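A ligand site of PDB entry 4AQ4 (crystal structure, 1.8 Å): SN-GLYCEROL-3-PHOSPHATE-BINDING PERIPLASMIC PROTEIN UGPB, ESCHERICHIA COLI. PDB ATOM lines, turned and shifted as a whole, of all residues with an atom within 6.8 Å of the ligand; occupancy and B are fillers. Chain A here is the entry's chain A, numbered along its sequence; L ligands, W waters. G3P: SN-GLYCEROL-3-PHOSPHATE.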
ATOM      1  N   MET A  14      -3.479 -26.635 -39.212  1.00  0.00           N
ATOM      2  CA  MET A  14      -3.556 -25.296 -38.616  1.00  0.00           C
ATOM      3  C   MET A  14      -4.706 -24.495 -39.227  1.00  0.00           C
ATOM      4  O   MET A  14      -4.646 -24.064 -40.366  1.00  0.00           O
ATOM      5  CB  MET A  14      -2.208 -24.565 -38.782  1.00  0.00           C
ATOM      6  CG  MET A  14      -1.000 -25.329 -38.205  1.00  0.00           C
ATOM      7  SD  MET A  14      -0.929 -25.297 -36.389  1.00  0.00           S
ATOM      8  CE  MET A  14      -1.909 -26.739 -35.953  1.00  0.00           C
ATOM      9  N   LEU A  18      -4.107 -19.586 -37.340  1.00  0.00           N
ATOM     10  CA  LEU A  18      -2.920 -20.442 -37.313  1.00  0.00           C
ATOM     11  C   LEU A  18      -2.461 -20.769 -38.724  1.00  0.00           C
ATOM     12  O   LEU A  18      -1.265 -20.714 -39.034  1.00  0.00           O
ATOM     13  CB  LEU A  18      -3.202 -21.728 -36.550  1.00  0.00           C
ATOM     14  CG  LEU A  18      -3.570 -21.517 -35.081  1.00  0.00           C
ATOM     15  CD1 LEU A  18      -3.922 -22.843 -34.418  1.00  0.00           C
ATOM     16  CD2 LEU A  18      -2.428 -20.838 -34.349  1.00  0.00           C
ATOM     17  N   TYR A  46      -6.482 -32.744 -36.715  1.00  0.00           N
ATOM     18  CA  TYR A  46      -5.284 -33.593 -36.614  1.00  0.00           C
ATOM     19  C   TYR A  46      -5.566 -35.061 -37.000  1.00  0.00           C
ATOM     20  O   TYR A  46      -4.704 -35.723 -37.594  1.00  0.00           O
ATOM     21  CB  TYR A  46      -4.758 -33.554 -35.174  1.00  0.00           C
ATOM     22  CG  TYR A  46      -3.931 -32.348 -34.786  1.00  0.00           C
ATOM     23  CD1 TYR A  46      -2.910 -31.866 -35.610  1.00  0.00           C
ATOM     24  CD2 TYR A  46      -4.155 -31.715 -33.571  1.00  0.00           C
ATOM     25  CE1 TYR A  46      -2.129 -30.768 -35.220  1.00  0.00           C
ATOM     26  CE2 TYR A  46      -3.393 -30.622 -33.178  1.00  0.00           C
ATOM     27  CZ  TYR A  46      -2.386 -30.166 -33.998  1.00  0.00           C
ATOM     28  OH  TYR A  46      -1.634 -29.103 -33.588  1.00  0.00           O
ATOM     29  N   GLN A  67       2.226 -32.693 -40.650  1.00  0.00           N
ATOM     30  CA  GLN A  67       2.055 -32.305 -39.240  1.00  0.00           C
ATOM     31  C   GLN A  67       1.215 -33.332 -38.498  1.00  0.00           C
ATOM     32  O   GLN A  67       0.046 -33.535 -38.835  1.00  0.00           O
ATOM     33  CB  GLN A  67       1.406 -30.912 -39.145  1.00  0.00           C
ATOM     34  CG  GLN A  67       1.267 -30.383 -37.709  1.00  0.00           C
ATOM     35  CD  GLN A  67       0.564 -29.045 -37.640  1.00  0.00           C
ATOM     36  OE1 GLN A  67      -0.463 -28.835 -38.317  1.00  0.00           O
ATOM     37  NE2 GLN A  67       1.074 -28.134 -36.798  1.00  0.00           N
ATOM     38  N   TYR A  69      -0.153 -34.687 -34.679  1.00  0.00           N
ATOM     39  CA  TYR A  69      -0.293 -34.305 -33.278  1.00  0.00           C
ATOM     40  C   TYR A  69       0.541 -35.170 -32.357  1.00  0.00           C
ATOM     41  O   TYR A  69       0.995 -36.269 -32.735  1.00  0.00           O
ATOM     42  CB  TYR A  69      -1.748 -34.230 -32.776  1.00  0.00           C
ATOM     43  CG  TYR A  69      -2.667 -35.440 -32.975  1.00  0.00           C
ATOM     44  CD1 TYR A  69      -2.293 -36.535 -33.748  1.00  0.00           C
ATOM     45  CD2 TYR A  69      -3.931 -35.451 -32.402  1.00  0.00           C
ATOM     46  CE1 TYR A  69      -3.171 -37.610 -33.941  1.00  0.00           C
ATOM     47  CE2 TYR A  69      -4.801 -36.507 -32.584  1.00  0.00           C
ATOM     48  CZ  TYR A  69      -4.420 -37.582 -33.345  1.00  0.00           C
ATOM     49  OH  TYR A  69      -5.299 -38.635 -33.516  1.00  0.00           O
ATOM     50  N   GLU A  70       0.742 -34.654 -31.145  1.00  0.00           N
ATOM     51  CA  GLU A  70       1.688 -35.234 -30.200  1.00  0.00           C
ATOM     52  C   GLU A  70       1.375 -36.706 -29.936  1.00  0.00           C
ATOM     53  O   GLU A  70       2.296 -37.517 -29.808  1.00  0.00           O
ATOM     54  CB  GLU A  70       1.684 -34.409 -28.893  1.00  0.00           C
ATOM     55  CG  GLU A  70       0.677 -34.833 -27.784  1.00  0.00           C
ATOM     56  CD  GLU A  70      -0.785 -34.426 -28.047  1.00  0.00           C
ATOM     57  OE1 GLU A  70      -1.267 -34.528 -29.206  1.00  0.00           O
ATOM     58  OE2 GLU A  70      -1.478 -34.022 -27.085  1.00  0.00           O
ATOM     59  N   VAL A  71       0.090 -37.049 -29.878  1.00  0.00           N
ATOM     60  CA  VAL A  71      -0.285 -38.408 -29.513  1.00  0.00           C
ATOM     61  C   VAL A  71       0.028 -39.420 -30.632  1.00  0.00           C
ATOM     62  O   VAL A  71       0.107 -40.626 -30.381  1.00  0.00           O
ATOM     63  CB  VAL A  71      -1.758 -38.498 -29.047  1.00  0.00           C
ATOM     64  CG1 VAL A  71      -1.942 -37.712 -27.745  1.00  0.00           C
ATOM     65  CG2 VAL A  71      -2.691 -37.979 -30.119  1.00  0.00           C
ATOM     66  N   ASN A 123       4.995 -26.706 -33.236  1.00  0.00           N
ATOM     67  CA  ASN A 123       3.920 -26.137 -32.435  1.00  0.00           C
ATOM     68  C   ASN A 123       3.634 -26.983 -31.202  1.00  0.00           C
ATOM     69  O   ASN A 123       2.952 -28.002 -31.276  1.00  0.00           O
ATOM     70  CB  ASN A 123       2.649 -25.913 -33.290  1.00  0.00           C
ATOM     71  CG  ASN A 123       2.065 -27.206 -33.846  1.00  0.00           C
ATOM     72  OD1 ASN A 123       2.759 -27.988 -34.493  1.00  0.00           O
ATOM     73  ND2 ASN A 123       0.774 -27.426 -33.591  1.00  0.00           N
ATOM     74  N   SER A 124       4.159 -26.557 -30.059  1.00  0.00           N
ATOM     75  CA  SER A 124       3.856 -27.228 -28.794  1.00  0.00           C
ATOM     76  C   SER A 124       3.021 -26.306 -27.919  1.00  0.00           C
ATOM     77  O   SER A 124       3.219 -25.092 -27.950  1.00  0.00           O
ATOM     78  CB  SER A 124       5.142 -27.609 -28.071  1.00  0.00           C
ATOM     79  OG  SER A 124       5.797 -28.672 -28.738  1.00  0.00           O
ATOM     80  N   SER A 125       2.107 -26.886 -27.151  1.00  0.00           N
ATOM     81  CA  SER A 125       1.208 -26.109 -26.310  1.00  0.00           C
ATOM     82  C   SER A 125       1.135 -26.732 -24.922  1.00  0.00           C
ATOM     83  O   SER A 125       1.593 -27.859 -24.718  1.00  0.00           O
ATOM     84  CB  SER A 125      -0.192 -26.188 -26.896  1.00  0.00           C
ATOM     85  OG  SER A 125      -0.549 -27.551 -27.028  1.00  0.00           O
ATOM     86  N   THR A 126       0.545 -25.999 -23.981  1.00  0.00           N
ATOM     87  CA  THR A 126      -0.052 -26.640 -22.809  1.00  0.00           C
ATOM     88  C   THR A 126      -1.468 -26.076 -22.705  1.00  0.00           C
ATOM     89  O   THR A 126      -1.757 -25.017 -23.288  1.00  0.00           O
ATOM     90  CB  THR A 126       0.752 -26.418 -21.490  1.00  0.00           C
ATOM     91  OG1 THR A 126       0.804 -25.034 -21.163  1.00  0.00           O
ATOM     92  CG2 THR A 126       2.163 -26.988 -21.626  1.00  0.00           C
ATOM     93  N   TRP A 173     -10.510 -30.449 -26.295  1.00  0.00           N
ATOM     94  CA  TRP A 173      -9.661 -31.659 -26.189  1.00  0.00           C
ATOM     95  C   TRP A 173      -9.745 -32.350 -24.833  1.00  0.00           C
ATOM     96  O   TRP A 173      -8.745 -32.419 -24.116  1.00  0.00           O
ATOM     97  CB  TRP A 173      -8.217 -31.305 -26.511  1.00  0.00           C
ATOM     98  CG  TRP A 173      -8.036 -30.797 -27.922  1.00  0.00           C
ATOM     99  CD1 TRP A 173      -8.083 -29.500 -28.337  1.00  0.00           C
ATOM    100  CD2 TRP A 173      -7.809 -31.587 -29.099  1.00  0.00           C
ATOM    101  NE1 TRP A 173      -7.880 -29.434 -29.707  1.00  0.00           N
ATOM    102  CE2 TRP A 173      -7.718 -30.701 -30.197  1.00  0.00           C
ATOM    103  CE3 TRP A 173      -7.669 -32.961 -29.328  1.00  0.00           C
ATOM    104  CZ2 TRP A 173      -7.481 -31.152 -31.498  1.00  0.00           C
ATOM    105  CZ3 TRP A 173      -7.424 -33.396 -30.626  1.00  0.00           C
ATOM    106  CH2 TRP A 173      -7.351 -32.497 -31.685  1.00  0.00           C
ATOM    107  N   TRP A 176      -7.017 -34.778 -23.577  1.00  0.00           N
ATOM    108  CA  TRP A 176      -5.737 -34.119 -23.339  1.00  0.00           C
ATOM    109  C   TRP A 176      -5.774 -33.307 -22.058  1.00  0.00           C
ATOM    110  O   TRP A 176      -4.827 -33.320 -21.266  1.00  0.00           O
ATOM    111  CB  TRP A 176      -5.428 -33.208 -24.528  1.00  0.00           C
ATOM    112  CG  TRP A 176      -4.147 -32.397 -24.427  1.00  0.00           C
ATOM    113  CD1 TRP A 176      -2.900 -32.870 -24.176  1.00  0.00           C
ATOM    114  CD2 TRP A 176      -4.019 -30.989 -24.649  1.00  0.00           C
ATOM    115  NE1 TRP A 176      -1.991 -31.828 -24.204  1.00  0.00           N
ATOM    116  CE2 TRP A 176      -2.661 -30.661 -24.488  1.00  0.00           C
ATOM    117  CE3 TRP A 176      -4.919 -29.975 -24.965  1.00  0.00           C
ATOM    118  CZ2 TRP A 176      -2.179 -29.359 -24.623  1.00  0.00           C
ATOM    119  CZ3 TRP A 176      -4.449 -28.667 -25.103  1.00  0.00           C
ATOM    120  CH2 TRP A 176      -3.093 -28.371 -24.936  1.00  0.00           C
ATOM    121  N   GLU A 180      -5.119 -36.572 -19.503  1.00  0.00           N
ATOM    122  CA  GLU A 180      -3.678 -36.605 -19.732  1.00  0.00           C
ATOM    123  C   GLU A 180      -3.006 -35.517 -18.902  1.00  0.00           C
ATOM    124  O   GLU A 180      -2.196 -35.794 -18.009  1.00  0.00           O
ATOM    125  CB  GLU A 180      -3.351 -36.458 -21.231  1.00  0.00           C
ATOM    126  CG  GLU A 180      -3.804 -37.649 -22.084  1.00  0.00           C
ATOM    127  CD  GLU A 180      -3.909 -37.341 -23.558  1.00  0.00           C
ATOM    128  OE1 GLU A 180      -3.198 -36.411 -24.039  1.00  0.00           O
ATOM    129  OE2 GLU A 180      -4.699 -38.021 -24.249  1.00  0.00           O
ATOM    130  N   ASP A 234     -11.550 -28.637 -30.757  1.00  0.00           N
ATOM    131  CA  ASP A 234     -11.439 -27.193 -30.486  1.00  0.00           C
ATOM    132  C   ASP A 234     -12.764 -26.440 -30.554  1.00  0.00           C
ATOM    133  O   ASP A 234     -12.750 -25.207 -30.654  1.00  0.00           O
ATOM    134  CB  ASP A 234     -10.456 -26.526 -31.451  1.00  0.00           C
ATOM    135  CG  ASP A 234      -9.060 -27.064 -31.331  1.00  0.00           C
ATOM    136  OD1 ASP A 234      -8.328 -26.651 -30.394  1.00  0.00           O
ATOM    137  OD2 ASP A 234      -8.680 -27.904 -32.183  1.00  0.00           O
ATOM    138  N   ALA A 250      -8.458 -24.616 -22.879  1.00  0.00           N
ATOM    139  CA  ALA A 250      -8.184 -24.905 -24.279  1.00  0.00           C
ATOM    140  C   ALA A 250      -6.686 -24.796 -24.519  1.00  0.00           C
ATOM    141  O   ALA A 250      -5.938 -24.356 -23.630  1.00  0.00           O
ATOM    142  CB  ALA A 250      -8.910 -23.907 -25.173  1.00  0.00           C
ATOM    143  N   SER A 251      -6.249 -25.211 -25.700  1.00  0.00           N
ATOM    144  CA  SER A 251      -4.841 -25.082 -26.071  1.00  0.00           C
ATOM    145  C   SER A 251      -4.367 -23.649 -25.947  1.00  0.00           C
ATOM    146  O   SER A 251      -5.089 -22.693 -26.286  1.00  0.00           O
ATOM    147  CB  SER A 251      -4.617 -25.545 -27.524  1.00  0.00           C
ATOM    148  OG  SER A 251      -3.268 -25.287 -27.926  1.00  0.00           O
ATOM    149  N   SER A 252      -3.130 -23.471 -25.497  1.00  0.00           N
ATOM    150  CA  SER A 252      -2.519 -22.156 -25.531  1.00  0.00           C
ATOM    151  C   SER A 252      -2.471 -21.640 -26.975  1.00  0.00           C
ATOM    152  O   SER A 252      -2.486 -20.432 -27.219  1.00  0.00           O
ATOM    153  CB  SER A 252      -1.144 -22.171 -24.861  1.00  0.00           C
ATOM    154  OG  SER A 252      -0.207 -22.943 -25.604  1.00  0.00           O
ATOM    155  N   GLY A 253      -2.432 -22.568 -27.934  1.00  0.00           N
ATOM    156  CA  GLY A 253      -2.462 -22.227 -29.349  1.00  0.00           C
ATOM    157  C   GLY A 253      -3.769 -21.654 -29.866  1.00  0.00           C
ATOM    158  O   GLY A 253      -3.854 -21.189 -31.005  1.00  0.00           O
ATOM    159  N   SER A 254      -4.804 -21.683 -29.022  1.00  0.00           N
ATOM    160  CA  SER A 254      -6.091 -21.077 -29.376  1.00  0.00           C
ATOM    161  C   SER A 254      -6.017 -19.549 -29.375  1.00  0.00           C
ATOM    162  O   SER A 254      -6.967 -18.878 -29.801  1.00  0.00           O
ATOM    163  CB  SER A 254      -7.165 -21.521 -28.377  1.00  0.00           C
ATOM    164  OG  SER A 254      -7.462 -22.902 -28.492  1.00  0.00           O
ATOM    165  N   ILE A 286       3.049 -31.502 -22.827  1.00  0.00           N
ATOM    166  CA  ILE A 286       2.746 -30.741 -24.022  1.00  0.00           C
ATOM    167  C   ILE A 286       1.638 -31.333 -24.858  1.00  0.00           C
ATOM    168  O   ILE A 286       1.373 -32.535 -24.831  1.00  0.00           O
ATOM    169  CB  ILE A 286       3.993 -30.498 -24.910  1.00  0.00           C
ATOM    170  CG1 ILE A 286       4.625 -31.820 -25.358  1.00  0.00           C
ATOM    171  CG2 ILE A 286       5.007 -29.662 -24.154  1.00  0.00           C
ATOM    172  CD1 ILE A 286       5.912 -31.623 -26.201  1.00  0.00           C
ATOM    173  N   GLY A 287       0.979 -30.457 -25.600  1.00  0.00           N
ATOM    174  CA  GLY A 287       0.129 -30.885 -26.694  1.00  0.00           C
ATOM    175  C   GLY A 287       0.663 -30.272 -27.972  1.00  0.00           C
ATOM    176  O   GLY A 287       1.833 -29.811 -28.044  1.00  0.00           O
ATOM    177  N   GLY A 288      -0.173 -30.231 -28.987  1.00  0.00           N
ATOM    178  CA  GLY A 288       0.242 -29.676 -30.253  1.00  0.00           C
ATOM    179  C   GLY A 288       0.706 -30.781 -31.172  1.00  0.00           C
ATOM    180  O   GLY A 288       0.111 -31.861 -31.194  1.00  0.00           O
ATOM    181  N   ALA A 289       1.770 -30.510 -31.931  1.00  0.00           N
ATOM    182  CA  ALA A 289       2.207 -31.418 -32.975  1.00  0.00           C
ATOM    183  C   ALA A 289       3.710 -31.326 -33.206  1.00  0.00           C
ATOM    184  O   ALA A 289       4.400 -30.527 -32.562  1.00  0.00           O
ATOM    185  CB  ALA A 289       1.450 -31.099 -34.277  1.00  0.00           C
ATOM    186  N   TYR A 327       1.174 -20.835 -29.064  1.00  0.00           N
ATOM    187  CA  TYR A 327       2.026 -22.003 -28.879  1.00  0.00           C
ATOM    188  C   TYR A 327       3.297 -21.550 -28.146  1.00  0.00           C
ATOM    189  O   TYR A 327       3.725 -20.405 -28.275  1.00  0.00           O
ATOM    190  CB  TYR A 327       2.370 -22.658 -30.212  1.00  0.00           C
ATOM    191  CG  TYR A 327       1.235 -23.441 -30.810  1.00  0.00           C
ATOM    192  CD1 TYR A 327       0.818 -24.645 -30.231  1.00  0.00           C
ATOM    193  CD2 TYR A 327       0.573 -23.007 -31.951  1.00  0.00           C
ATOM    194  CE1 TYR A 327      -0.247 -25.375 -30.770  1.00  0.00           C
ATOM    195  CE2 TYR A 327      -0.473 -23.742 -32.511  1.00  0.00           C
ATOM    196  CZ  TYR A 327      -0.873 -24.918 -31.913  1.00  0.00           C
ATOM    197  OH  TYR A 327      -1.900 -25.643 -32.467  1.00  0.00           O
ATOM    198  N   ARG A 378      -7.415 -42.179 -28.036  1.00  0.00           N
ATOM    199  CA  ARG A 378      -8.112 -40.895 -27.893  1.00  0.00           C
ATOM    200  C   ARG A 378      -9.586 -41.026 -28.256  1.00  0.00           C
ATOM    201  O   ARG A 378     -10.447 -40.446 -27.595  1.00  0.00           O
ATOM    202  CB  ARG A 378      -7.466 -39.814 -28.769  1.00  0.00           C
ATOM    203  CG  ARG A 378      -6.252 -39.122 -28.149  1.00  0.00           C
ATOM    204  CD  ARG A 378      -6.717 -38.050 -27.156  1.00  0.00           C
ATOM    205  NE  ARG A 378      -5.618 -37.252 -26.621  1.00  0.00           N
ATOM    206  CZ  ARG A 378      -5.088 -36.200 -27.249  1.00  0.00           C
ATOM    207  NH1 ARG A 378      -5.536 -35.829 -28.446  1.00  0.00           N
ATOM    208  NH2 ARG A 378      -4.100 -35.513 -26.673  1.00  0.00           N
HETATM  209  O1  G3P L   1      -3.834 -33.822 -29.396  1.00  0.00           O
HETATM  210  C1  G3P L   1      -3.975 -32.447 -29.644  1.00  0.00           C
HETATM  211  C2  G3P L   1      -3.886 -31.534 -28.456  1.00  0.00           C
HETATM  212  O2  G3P L   1      -2.607 -31.585 -27.909  1.00  0.00           O
HETATM  213  C3  G3P L   1      -4.151 -30.106 -28.862  1.00  0.00           C
HETATM  214  O1P G3P L   1      -3.325 -29.598 -29.872  1.00  0.00           O
HETATM  215  O4P G3P L   1      -4.553 -27.462 -30.191  1.00  0.00           O
HETATM  216  O2P G3P L   1      -2.430 -27.856 -31.381  1.00  0.00           O
HETATM  217  O3P G3P L   1      -2.426 -27.455 -28.898  1.00  0.00           O
HETATM  218  P   G3P L   1      -3.172 -28.064 -30.070  1.00  0.00           P
HETATM  219  O   HOH W   1      -4.597 -24.534 -31.110  1.00  0.00           O
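The side-chain hydroxyl of Ser 251 is in hydrogen-bond range of an oxygen (O3P) of the ligand. An oxygen (O1) of the ligand lies within hydrogen-bond range of the guanidinium group (NH1) of Arg 378, 2.8 Å away. An oxygen (O2P) of the ligand is in hydrogen-bond range of the side-chain hydroxyl (OH) of Tyr 327, 2.5 Å away. OH of Tyr 46 sits at hydrogen-bond distance from O2P of the ligand. OG of Ser 125 lies within hydrogen-bond range of O3P of the ligand, 2.7 Å away. The backbone NH (N) of Gly 288 is in hydrogen-bond range of an oxygen (O2) of the ligand, at 3.0 Å. OE1 of Glu 70 sits at hydrogen-bond distance from O1 of the ligand.
O of Ser 125 is in hydrogen-bond range of N of Gly 287 (2.8 Å). The side-chain hydroxyl (OG) of Ser 251 sits at hydrogen-bond distance from the backbone NH (N) of Gly 253. NE1 of Trp 176 is in hydrogen-bond range of O of Ile 286, 3.5 Å away. OG of Ser 125 is in hydrogen-bond range of N of Gly 288. NE2 of Gln 67 is in hydrogen-bond range of OD1 of Asn 123 (2.9 Å). The backbone NH (N) of Glu 70 sits at hydrogen-bond distance from the backbone carbonyl oxygen (O) of Gly 288, at 2.9 Å. OH of Tyr 46 lies within hydrogen-bond range of ND2 of Asn 123. The guanidinium group of Arg 378 is in salt-bridge range of the side-chain carboxylate of Glu 180 (2.7 Å).
Tyr 69 touches the ligand. Asn 123 touches the ligand (ND2 to O2P, 3.9 Å). Trp 173 touches the ligand (CZ3 to C1, 3.7 Å). Trp 176 touches the ligand. OD1 of Asp 234 touches O4P of the ligand, 3.9 Å away. Gly 287 touches the ligand.
Water W1 lies within hydrogen-bond range of O4P of the ligand, OH of Tyr 327 and O of Gly 253.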
